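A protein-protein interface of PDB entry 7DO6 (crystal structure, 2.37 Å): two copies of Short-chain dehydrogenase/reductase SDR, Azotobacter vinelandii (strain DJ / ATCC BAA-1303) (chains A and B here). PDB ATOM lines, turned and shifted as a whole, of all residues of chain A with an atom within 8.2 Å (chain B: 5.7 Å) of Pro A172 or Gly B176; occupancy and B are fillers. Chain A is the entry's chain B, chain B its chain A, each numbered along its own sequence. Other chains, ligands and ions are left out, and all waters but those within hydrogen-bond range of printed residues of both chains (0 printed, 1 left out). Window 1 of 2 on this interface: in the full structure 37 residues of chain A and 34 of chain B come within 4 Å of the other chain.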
ATOM      1  N   TYR A 121      17.697 -14.959 -37.572  1.00  0.00           N
ATOM      2  CA  TYR A 121      18.181 -15.096 -36.204  1.00  0.00           C
ATOM      3  C   TYR A 121      19.685 -15.332 -36.178  1.00  0.00           C
ATOM      4  O   TYR A 121      20.399 -14.754 -35.350  1.00  0.00           O
ATOM      5  CB  TYR A 121      17.450 -16.240 -35.497  1.00  0.00           C
ATOM      6  CG  TYR A 121      18.026 -16.611 -34.140  1.00  0.00           C
ATOM      7  CD1 TYR A 121      17.609 -15.961 -32.983  1.00  0.00           C
ATOM      8  CD2 TYR A 121      18.978 -17.613 -34.018  1.00  0.00           C
ATOM      9  CE1 TYR A 121      18.130 -16.296 -31.746  1.00  0.00           C
ATOM     10  CE2 TYR A 121      19.505 -17.953 -32.791  1.00  0.00           C
ATOM     11  CZ  TYR A 121      19.077 -17.295 -31.657  1.00  0.00           C
ATOM     12  OH  TYR A 121      19.604 -17.639 -30.434  1.00  0.00           O
ATOM     13  N   THR A 124      21.667 -12.263 -36.758  1.00  0.00           N
ATOM     14  CA  THR A 124      21.521 -11.343 -35.636  1.00  0.00           C
ATOM     15  C   THR A 124      22.466 -11.712 -34.497  1.00  0.00           C
ATOM     16  O   THR A 124      23.268 -10.889 -34.043  1.00  0.00           O
ATOM     17  CB  THR A 124      20.068 -11.345 -35.156  1.00  0.00           C
ATOM     18  OG1 THR A 124      19.206 -10.942 -36.230  1.00  0.00           O
ATOM     19  CG2 THR A 124      19.892 -10.402 -33.980  1.00  0.00           C
ATOM     20  N   VAL A 125      22.381 -12.960 -34.026  1.00  0.00           N
ATOM     21  CA  VAL A 125      23.244 -13.423 -32.942  1.00  0.00           C
ATOM     22  C   VAL A 125      24.701 -13.457 -33.390  1.00  0.00           C
ATOM     23  O   VAL A 125      25.608 -13.122 -32.619  1.00  0.00           O
ATOM     24  CB  VAL A 125      22.773 -14.805 -32.445  1.00  0.00           C
ATOM     25  CG1 VAL A 125      23.691 -15.333 -31.341  1.00  0.00           C
ATOM     26  CG2 VAL A 125      21.333 -14.732 -31.963  1.00  0.00           C
ATOM     27  N   ASN A 128      25.928  -9.653 -33.440  1.00  0.00           N
ATOM     28  CA  ASN A 128      25.845  -8.886 -32.201  1.00  0.00           C
ATOM     29  C   ASN A 128      26.634  -9.528 -31.067  1.00  0.00           C
ATOM     30  O   ASN A 128      27.242  -8.820 -30.257  1.00  0.00           O
ATOM     31  CB  ASN A 128      24.383  -8.715 -31.789  1.00  0.00           C
ATOM     32  CG  ASN A 128      23.589  -7.893 -32.780  1.00  0.00           C
ATOM     33  OD1 ASN A 128      24.114  -7.470 -33.810  1.00  0.00           O
ATOM     34  ND2 ASN A 128      22.317  -7.662 -32.476  1.00  0.00           N
ATOM     35  N   LEU A 129      26.640 -10.858 -30.987  1.00  0.00           N
ATOM     36  CA  LEU A 129      27.197 -11.570 -29.844  1.00  0.00           C
ATOM     37  C   LEU A 129      28.450 -12.363 -30.195  1.00  0.00           C
ATOM     38  O   LEU A 129      29.515 -12.123 -29.617  1.00  0.00           O
ATOM     39  CB  LEU A 129      26.127 -12.493 -29.250  1.00  0.00           C
ATOM     40  CG  LEU A 129      26.466 -13.194 -27.937  1.00  0.00           C
ATOM     41  CD1 LEU A 129      26.793 -12.179 -26.855  1.00  0.00           C
ATOM     42  CD2 LEU A 129      25.312 -14.083 -27.513  1.00  0.00           C
ATOM     43  N   SER A 156      25.730  -1.968 -25.580  1.00  0.00           N
ATOM     44  CA  SER A 156      24.565  -2.841 -25.472  1.00  0.00           C
ATOM     45  C   SER A 156      23.305  -1.986 -25.622  1.00  0.00           C
ATOM     46  O   SER A 156      23.267  -1.166 -26.546  1.00  0.00           O
ATOM     47  CB  SER A 156      24.666  -3.655 -24.182  1.00  0.00           C
ATOM     48  OG  SER A 156      23.421  -4.248 -23.847  1.00  0.00           O
ATOM     49  N   SER A 159      17.371  -2.585 -23.929  1.00  0.00           N
ATOM     50  CA  SER A 159      16.742  -3.876 -24.176  1.00  0.00           C
ATOM     51  C   SER A 159      17.490  -5.034 -23.531  1.00  0.00           C
ATOM     52  O   SER A 159      17.027  -6.176 -23.632  1.00  0.00           O
ATOM     53  CB  SER A 159      16.606  -4.114 -25.681  1.00  0.00           C
ATOM     54  OG  SER A 159      15.492  -3.411 -26.207  1.00  0.00           O
ATOM     55  N   ALA A 160      18.626  -4.778 -22.880  1.00  0.00           N
ATOM     56  CA  ALA A 160      19.278  -5.800 -22.071  1.00  0.00           C
ATOM     57  C   ALA A 160      18.567  -6.038 -20.746  1.00  0.00           C
ATOM     58  O   ALA A 160      18.930  -6.975 -20.026  1.00  0.00           O
ATOM     59  CB  ALA A 160      20.736  -5.417 -21.809  1.00  0.00           C
ATOM     60  N   VAL A 162      14.804  -5.317 -20.517  1.00  0.00           N
ATOM     61  CA  VAL A 162      13.370  -5.380 -20.757  1.00  0.00           C
ATOM     62  C   VAL A 162      13.127  -6.146 -22.054  1.00  0.00           C
ATOM     63  O   VAL A 162      14.064  -6.562 -22.741  1.00  0.00           O
ATOM     64  CB  VAL A 162      12.726  -3.979 -20.815  1.00  0.00           C
ATOM     65  CG1 VAL A 162      12.677  -3.364 -19.426  1.00  0.00           C
ATOM     66  CG2 VAL A 162      13.498  -3.081 -21.763  1.00  0.00           C
ATOM     67  N   GLY A 164      11.042  -6.949 -25.895  1.00  0.00           N
ATOM     68  CA  GLY A 164      10.603  -6.330 -27.131  1.00  0.00           C
ATOM     69  C   GLY A 164       9.943  -7.343 -28.042  1.00  0.00           C
ATOM     70  O   GLY A 164      10.609  -8.257 -28.534  1.00  0.00           O
ATOM     71  N   GLN A 167      11.569  -7.968 -31.142  1.00  0.00           N
ATOM     72  CA  GLN A 167      13.013  -8.054 -30.965  1.00  0.00           C
ATOM     73  C   GLN A 167      13.404  -9.315 -30.203  1.00  0.00           C
ATOM     74  O   GLN A 167      14.417  -9.329 -29.500  1.00  0.00           O
ATOM     75  CB  GLN A 167      13.548  -6.812 -30.251  1.00  0.00           C
ATOM     76  CG  GLN A 167      13.230  -5.501 -30.956  1.00  0.00           C
ATOM     77  CD  GLN A 167      13.409  -4.294 -30.057  1.00  0.00           C
ATOM     78  OE1 GLN A 167      12.456  -3.823 -29.436  1.00  0.00           O
ATOM     79  NE2 GLN A 167      14.634  -3.782 -29.987  1.00  0.00           N
ATOM     80  N   THR A 168      12.609 -10.384 -30.338  1.00  0.00           N
ATOM     81  CA  THR A 168      12.874 -11.617 -29.598  1.00  0.00           C
ATOM     82  C   THR A 168      14.252 -12.182 -29.914  1.00  0.00           C
ATOM     83  O   THR A 168      14.895 -12.779 -29.043  1.00  0.00           O
ATOM     84  CB  THR A 168      11.798 -12.661 -29.903  1.00  0.00           C
ATOM     85  OG1 THR A 168      11.583 -12.726 -31.319  1.00  0.00           O
ATOM     86  CG2 THR A 168      10.489 -12.302 -29.212  1.00  0.00           C
ATOM     87  N   HIS A 169      14.718 -12.011 -31.148  1.00  0.00           N
ATOM     88  CA  HIS A 169      16.070 -12.402 -31.523  1.00  0.00           C
ATOM     89  C   HIS A 169      17.111 -11.376 -31.100  1.00  0.00           C
ATOM     90  O   HIS A 169      18.299 -11.711 -31.025  1.00  0.00           O
ATOM     91  CB  HIS A 169      16.147 -12.594 -33.038  1.00  0.00           C
ATOM     92  CG  HIS A 169      15.835 -11.350 -33.810  1.00  0.00           C
ATOM     93  ND1 HIS A 169      14.663 -10.645 -33.642  1.00  0.00           N
ATOM     94  CD2 HIS A 169      16.548 -10.675 -34.743  1.00  0.00           C
ATOM     95  CE1 HIS A 169      14.664  -9.594 -34.442  1.00  0.00           C
ATOM     96  NE2 HIS A 169      15.796  -9.590 -35.121  1.00  0.00           N
ATOM     97  N   TYR A 170      16.694 -10.141 -30.827  1.00  0.00           N
ATOM     98  CA  TYR A 170      17.613  -9.031 -30.615  1.00  0.00           C
ATOM     99  C   TYR A 170      18.014  -8.871 -29.152  1.00  0.00           C
ATOM    100  O   TYR A 170      19.206  -8.762 -28.846  1.00  0.00           O
ATOM    101  CB  TYR A 170      16.982  -7.735 -31.132  1.00  0.00           C
ATOM    102  CG  TYR A 170      17.809  -6.500 -30.868  1.00  0.00           C
ATOM    103  CD1 TYR A 170      19.059  -6.340 -31.450  1.00  0.00           C
ATOM    104  CD2 TYR A 170      17.335  -5.489 -30.045  1.00  0.00           C
ATOM    105  CE1 TYR A 170      19.816  -5.209 -31.215  1.00  0.00           C
ATOM    106  CE2 TYR A 170      18.082  -4.353 -29.806  1.00  0.00           C
ATOM    107  CZ  TYR A 170      19.322  -4.217 -30.393  1.00  0.00           C
ATOM    108  OH  TYR A 170      20.072  -3.087 -30.157  1.00  0.00           O
ATOM    109  N   THR A 171      17.039  -8.852 -28.241  1.00  0.00           N
ATOM    110  CA  THR A 171      17.355  -8.599 -26.837  1.00  0.00           C
ATOM    111  C   THR A 171      18.308  -9.622 -26.219  1.00  0.00           C
ATOM    112  O   THR A 171      19.168  -9.203 -25.425  1.00  0.00           O
ATOM    113  CB  THR A 171      16.062  -8.486 -26.015  1.00  0.00           C
ATOM    114  OG1 THR A 171      15.321  -9.710 -26.074  1.00  0.00           O
ATOM    115  CG2 THR A 171      15.194  -7.356 -26.541  1.00  0.00           C
ATOM    116  N   PRO A 172      18.238 -10.931 -26.518  1.00  0.00           N
ATOM    117  CA  PRO A 172      19.241 -11.842 -25.937  1.00  0.00           C
ATOM    118  C   PRO A 172      20.663 -11.510 -26.349  1.00  0.00           C
ATOM    119  O   PRO A 172      21.593 -11.733 -25.564  1.00  0.00           O
ATOM    120  CB  PRO A 172      18.809 -13.222 -26.458  1.00  0.00           C
ATOM    121  CG  PRO A 172      17.361 -13.077 -26.747  1.00  0.00           C
ATOM    122  CD  PRO A 172      17.229 -11.683 -27.285  1.00  0.00           C
ATOM    123  N   THR A 173      20.863 -10.982 -27.557  1.00  0.00           N
ATOM    124  CA  THR A 173      22.202 -10.575 -27.967  1.00  0.00           C
ATOM    125  C   THR A 173      22.719  -9.433 -27.099  1.00  0.00           C
ATOM    126  O   THR A 173      23.900  -9.403 -26.733  1.00  0.00           O
ATOM    127  CB  THR A 173      22.203 -10.161 -29.439  1.00  0.00           C
ATOM    128  OG1 THR A 173      21.556  -8.889 -29.578  1.00  0.00           O
ATOM    129  CG2 THR A 173      21.477 -11.190 -30.291  1.00  0.00           C
ATOM    130  N   LYS A 174      21.846  -8.482 -26.762  1.00  0.00           N
ATOM    131  CA  LYS A 174      22.266  -7.346 -25.949  1.00  0.00           C
ATOM    132  C   LYS A 174      22.387  -7.725 -24.479  1.00  0.00           C
ATOM    133  O   LYS A 174      23.328  -7.295 -23.802  1.00  0.00           O
ATOM    134  CB  LYS A 174      21.290  -6.184 -26.136  1.00  0.00           C
ATOM    135  CG  LYS A 174      20.938  -5.897 -27.594  1.00  0.00           C
ATOM    136  CD  LYS A 174      21.877  -4.867 -28.200  1.00  0.00           C
ATOM    137  CE  LYS A 174      23.104  -5.513 -28.820  1.00  0.00           C
ATOM    138  NZ  LYS A 174      24.033  -4.500 -29.390  1.00  0.00           N
ATOM    139  N   ALA A 175      21.450  -8.525 -23.968  1.00  0.00           N
ATOM    140  CA  ALA A 175      21.599  -9.054 -22.617  1.00  0.00           C
ATOM    141  C   ALA A 175      22.847  -9.916 -22.494  1.00  0.00           C
ATOM    142  O   ALA A 175      23.477  -9.948 -21.430  1.00  0.00           O
ATOM    143  CB  ALA A 175      20.358  -9.855 -22.224  1.00  0.00           C
ATOM    144  N   GLY A 176      23.223 -10.615 -23.570  1.00  0.00           N
ATOM    145  CA  GLY A 176      24.411 -11.449 -23.530  1.00  0.00           C
ATOM    146  C   GLY A 176      25.698 -10.654 -23.584  1.00  0.00           C
ATOM    147  O   GLY A 176      26.722 -11.087 -23.044  1.00  0.00           O
ATOM    148  N   LEU A 177      25.670  -9.487 -24.233  1.00  0.00           N
ATOM    149  CA  LEU A 177      26.844  -8.621 -24.248  1.00  0.00           C
ATOM    150  C   LEU A 177      27.117  -8.044 -22.866  1.00  0.00           C
ATOM    151  O   LEU A 177      28.278  -7.895 -22.468  1.00  0.00           O
ATOM    152  CB  LEU A 177      26.663  -7.504 -25.273  1.00  0.00           C
ATOM    153  CG  LEU A 177      27.253  -7.788 -26.653  1.00  0.00           C
ATOM    154  CD1 LEU A 177      26.912  -6.663 -27.612  1.00  0.00           C
ATOM    155  CD2 LEU A 177      28.760  -7.982 -26.548  1.00  0.00           C
ATOM    156  N   LEU A 178      26.061  -7.706 -22.123  1.00  0.00           N
ATOM    157  CA  LEU A 178      26.234  -7.336 -20.722  1.00  0.00           C
ATOM    158  C   LEU A 178      26.842  -8.491 -19.937  1.00  0.00           C
ATOM    159  O   LEU A 178      27.851  -8.324 -19.242  1.00  0.00           O
ATOM    160  CB  LEU A 178      24.892  -6.917 -20.122  1.00  0.00           C
ATOM    161  CG  LEU A 178      24.871  -5.811 -19.061  1.00  0.00           C
ATOM    162  CD1 LEU A 178      23.437  -5.400 -18.766  1.00  0.00           C
ATOM    163  CD2 LEU A 178      25.571  -6.236 -17.782  1.00  0.00           C
ATOM    164  N   SER A 179      26.248  -9.683 -20.059  1.00  0.00           N
ATOM    165  CA  SER A 179      26.764 -10.852 -19.353  1.00  0.00           C
ATOM    166  C   SER A 179      28.192 -11.174 -19.766  1.00  0.00           C
ATOM    167  O   SER A 179      28.947 -11.767 -18.987  1.00  0.00           O
ATOM    168  CB  SER A 179      25.859 -12.054 -19.608  1.00  0.00           C
ATOM    169  OG  SER A 179      26.304 -13.177 -18.869  1.00  0.00           O
ATOM    170  N   LEU B 129      21.249 -21.586 -26.410  1.00  0.00           N
ATOM    171  CA  LEU B 129      20.380 -20.470 -26.775  1.00  0.00           C
ATOM    172  C   LEU B 129      19.717 -20.636 -28.135  1.00  0.00           C
ATOM    173  O   LEU B 129      18.487 -20.518 -28.234  1.00  0.00           O
ATOM    174  CB  LEU B 129      21.172 -19.151 -26.740  1.00  0.00           C
ATOM    175  CG  LEU B 129      20.368 -17.875 -27.021  1.00  0.00           C
ATOM    176  CD1 LEU B 129      19.361 -17.602 -25.910  1.00  0.00           C
ATOM    177  CD2 LEU B 129      21.288 -16.678 -27.215  1.00  0.00           C
ATOM    178  N   THR B 171      27.669 -17.835 -19.575  1.00  0.00           N
ATOM    179  CA  THR B 171      26.733 -16.886 -18.978  1.00  0.00           C
ATOM    180  C   THR B 171      25.957 -16.041 -19.991  1.00  0.00           C
ATOM    181  O   THR B 171      24.805 -15.689 -19.682  1.00  0.00           O
ATOM    182  CB  THR B 171      27.459 -15.974 -17.969  1.00  0.00           C
ATOM    183  OG1 THR B 171      28.196 -14.955 -18.656  1.00  0.00           O
ATOM    184  CG2 THR B 171      28.400 -16.778 -17.088  1.00  0.00           C
ATOM    185  N   PRO B 172      26.484 -15.682 -21.171  1.00  0.00           N
ATOM    186  CA  PRO B 172      25.624 -14.978 -22.138  1.00  0.00           C
ATOM    187  C   PRO B 172      24.444 -15.807 -22.611  1.00  0.00           C
ATOM    188  O   PRO B 172      23.392 -15.239 -22.928  1.00  0.00           O
ATOM    189  CB  PRO B 172      26.586 -14.649 -23.290  1.00  0.00           C
ATOM    190  CG  PRO B 172      27.928 -14.620 -22.658  1.00  0.00           C
ATOM    191  CD  PRO B 172      27.883 -15.715 -21.638  1.00  0.00           C
ATOM    192  N   THR B 173      24.576 -17.136 -22.664  1.00  0.00           N
ATOM    193  CA  THR B 173      23.433 -17.954 -23.062  1.00  0.00           C
ATOM    194  C   THR B 173      22.393 -18.018 -21.951  1.00  0.00           C
ATOM    195  O   THR B 173      21.187 -18.047 -22.225  1.00  0.00           O
ATOM    196  CB  THR B 173      23.888 -19.362 -23.455  1.00  0.00           C
ATOM    197  OG1 THR B 173      24.250 -20.106 -22.284  1.00  0.00           O
ATOM    198  CG2 THR B 173      25.075 -19.301 -24.412  1.00  0.00           C
ATOM    199  N   LYS B 174      22.839 -18.035 -20.692  1.00  0.00           N
ATOM    200  CA  LYS B 174      21.899 -17.999 -19.574  1.00  0.00           C
ATOM    201  C   LYS B 174      21.152 -16.670 -19.533  1.00  0.00           C
ATOM    202  O   LYS B 174      19.918 -16.642 -19.460  1.00  0.00           O
ATOM    203  CB  LYS B 174      22.636 -18.246 -18.257  1.00  0.00           C
ATOM    204  CG  LYS B 174      23.234 -19.635 -18.127  1.00  0.00           C
ATOM    205  CD  LYS B 174      22.160 -20.700 -18.234  1.00  0.00           C
ATOM    206  CE  LYS B 174      22.428 -21.641 -19.394  1.00  0.00           C
ATOM    207  NZ  LYS B 174      21.300 -22.592 -19.580  1.00  0.00           N
ATOM    208  N   ALA B 175      21.889 -15.556 -19.577  1.00  0.00           N
ATOM    209  CA  ALA B 175      21.245 -14.248 -19.646  1.00  0.00           C
ATOM    210  C   ALA B 175      20.458 -14.079 -20.938  1.00  0.00           C
ATOM    211  O   ALA B 175      19.428 -13.394 -20.951  1.00  0.00           O
ATOM    212  CB  ALA B 175      22.287 -13.136 -19.510  1.00  0.00           C
ATOM    213  N   GLY B 176      20.923 -14.693 -22.031  1.00  0.00           N
ATOM    214  CA  GLY B 176      20.152 -14.664 -23.263  1.00  0.00           C
ATOM    215  C   GLY B 176      18.824 -15.384 -23.128  1.00  0.00           C
ATOM    216  O   GLY B 176      17.805 -14.931 -23.656  1.00  0.00           O
ATOM    217  N   LEU B 177      18.820 -16.513 -22.409  1.00  0.00           N
ATOM    218  CA  LEU B 177      17.579 -17.240 -22.158  1.00  0.00           C
ATOM    219  C   LEU B 177      16.611 -16.405 -21.331  1.00  0.00           C
ATOM    220  O   LEU B 177      15.397 -16.439 -21.561  1.00  0.00           O
ATOM    221  CB  LEU B 177      17.877 -18.560 -21.443  1.00  0.00           C
ATOM    222  CG  LEU B 177      17.786 -19.874 -22.220  1.00  0.00           C
ATOM    223  CD1 LEU B 177      17.970 -21.049 -21.271  1.00  0.00           C
ATOM    224  CD2 LEU B 177      16.465 -19.983 -22.968  1.00  0.00           C
ATOM    225  N   LEU B 178      17.130 -15.661 -20.350  1.00  0.00           N
ATOM    226  CA  LEU B 178      16.275 -14.802 -19.539  1.00  0.00           C
ATOM    227  C   LEU B 178      15.672 -13.681 -20.378  1.00  0.00           C
ATOM    228  O   LEU B 178      14.480 -13.378 -20.254  1.00  0.00           O
ATOM    229  CB  LEU B 178      17.071 -14.234 -18.363  1.00  0.00           C
ATOM    230  CG  LEU B 178      16.298 -13.558 -17.228  1.00  0.00           C
ATOM    231  CD1 LEU B 178      16.918 -13.893 -15.883  1.00  0.00           C
ATOM    232  CD2 LEU B 178      16.266 -12.059 -17.427  1.00  0.00           C
ATOM    233  N   SER B 179      16.483 -13.057 -21.238  1.00  0.00           N
ATOM    234  CA  SER B 179      15.975 -12.005 -22.113  1.00  0.00           C
ATOM    235  C   SER B 179      14.889 -12.530 -23.046  1.00  0.00           C
ATOM    236  O   SER B 179      13.901 -11.833 -23.309  1.00  0.00           O
ATOM    237  CB  SER B 179      17.122 -11.402 -22.921  1.00  0.00           C
ATOM    238  OG  SER B 179      16.848 -10.059 -23.268  1.00  0.00           O
ATOM    239  N   LEU B 180      15.057 -13.755 -23.555  1.00  0.00           N
ATOM    240  CA  LEU B 180      14.060 -14.334 -24.451  1.00  0.00           C
ATOM    241  C   LEU B 180      12.700 -14.441 -23.774  1.00  0.00           C
ATOM    242  O   LEU B 180      11.669 -14.131 -24.384  1.00  0.00           O
ATOM    243  CB  LEU B 180      14.525 -15.708 -24.935  1.00  0.00           C
ATOM    244  CG  LEU B 180      13.707 -16.339 -26.064  1.00  0.00           C
ATOM    245  CD1 LEU B 180      13.624 -15.392 -27.251  1.00  0.00           C
ATOM    246  CD2 LEU B 180      14.301 -17.677 -26.483  1.00  0.00           C
ATOM    247  N   MET B 181      12.679 -14.878 -22.511  1.00  0.00           N
ATOM    248  CA  MET B 181      11.419 -14.978 -21.780  1.00  0.00           C
ATOM    249  C   MET B 181      10.772 -13.614 -21.583  1.00  0.00           C
ATOM    250  O   MET B 181       9.542 -13.516 -21.516  1.00  0.00           O
ATOM    251  CB  MET B 181      11.649 -15.657 -20.429  1.00  0.00           C
ATOM    252  CG  MET B 181      12.132 -17.095 -20.530  1.00  0.00           C
ATOM    253  SD  MET B 181      10.929 -18.157 -21.347  1.00  0.00           S
ATOM    254  CE  MET B 181      11.626 -18.272 -23.002  1.00  0.00           C
ATOM    255  N   SER B 183      11.003 -10.943 -23.775  1.00  0.00           N
ATOM    256  CA  SER B 183      10.487 -10.494 -25.070  1.00  0.00           C
ATOM    257  C   SER B 183       9.303 -11.324 -25.531  1.00  0.00           C
ATOM    258  O   SER B 183       8.295 -10.778 -25.990  1.00  0.00           O
ATOM    259  CB  SER B 183      11.598 -10.541 -26.123  1.00  0.00           C
ATOM    260  OG  SER B 183      12.661  -9.675 -25.795  1.00  0.00           O
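Of the 13 printed residues of chain B, 8 touch a printed residue of chain A. Printed residues of chain A that touch a printed residue of chain B: Tyr A121, Ser A159, Gly A164, Thr A168, Thr A171, Pro A172, Ala A175, Gly A176 and Ser A179. Among the printed residues, 16 pairs touch across the chains. Among the printed residues, no Asp or Glu carboxylate lies within 4 Å of a Lys or Arg side-chain nitrogen of the other chain.
Thr A171 touches Ser B179, and with the chains exchanged Ser A179 touches Thr B171. Pro A172 touches Gly B176, and with the chains exchanged Gly A176 touches Pro B172. Pro A172 touches Ser B179, and with the chains exchanged Ser A179 touches Pro B172. Ala A175 touches its own counterpart, Ala B175. Positions printed for both chains: 129, 171, 172, 173, 174, 175, 176, 177, 178 and 179. Of the 16 pairs that touch across the chains among the printed residues, 9 have their exchanged pair printed and touching as well.
Printed residues of chain B within 4 Å of Tyr A121: Leu B129. Printed residues of chain B within 4 Å of Gly A164: Ser B183 (3.2 Å). Of the printed residues of chain B, Thr A171 touches Ser B179 (3.2 Å) and Ser B183 (2.7 Å). Printed residues of chain A within 4 Å of Pro B172: Gly A176 and Ser A179. Ala B175 touches just these residues of chain A: Ala A175 (3.9 Å) and Ser A179 (3.7 Å). Of chain A, only Pro A172 (3.4 Å) comes within 4 Å of Gly B176. Of the printed residues of chain A, Ser B183 touches Gly A164 (3.2 Å), Thr A168 (3.7 Å) and Thr A171 (2.7 Å). The nearest residue of chain A that does not touch Gly B176 is Ala A175 (4.9 Å).
Among the printed residues, merely in contact across the chains: Thr A168 with Leu B180, Pro A172 with Gly B176, Tyr A121 with Leu B129, Gly A176 with Pro B172, Pro A172 with Ser B179, Ala A175 with Ser B179, Thr A168 with Ser B183, Ser A179 with Ala B175, Ala A175 with Ala B175, Ser A159 with Ser B179 and Pro A172 with Leu B180.
The side-chain hydroxyl of Ser A179 sits at hydrogen-bond distance from the side-chain hydroxyl of Thr B171. The side-chain hydroxyl of Ser A179 sits close to the backbone nitrogen of Pro B172, at 3.4 Å. The backbone NH (N) of Gly A164 is in hydrogen-bond range of the side-chain hydroxyl (OG) of Ser B183, at 3.2 Å. The side-chain hydroxyl (OG) of Ser B179 is in hydrogen-bond range of the side-chain hydroxyl (OG1) of Thr A171 (3.2 Å). The side-chain hydroxyl (OG1) of Thr A171 sits at hydrogen-bond distance from the side-chain hydroxyl (OG) of Ser B183, at 2.7 Å.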
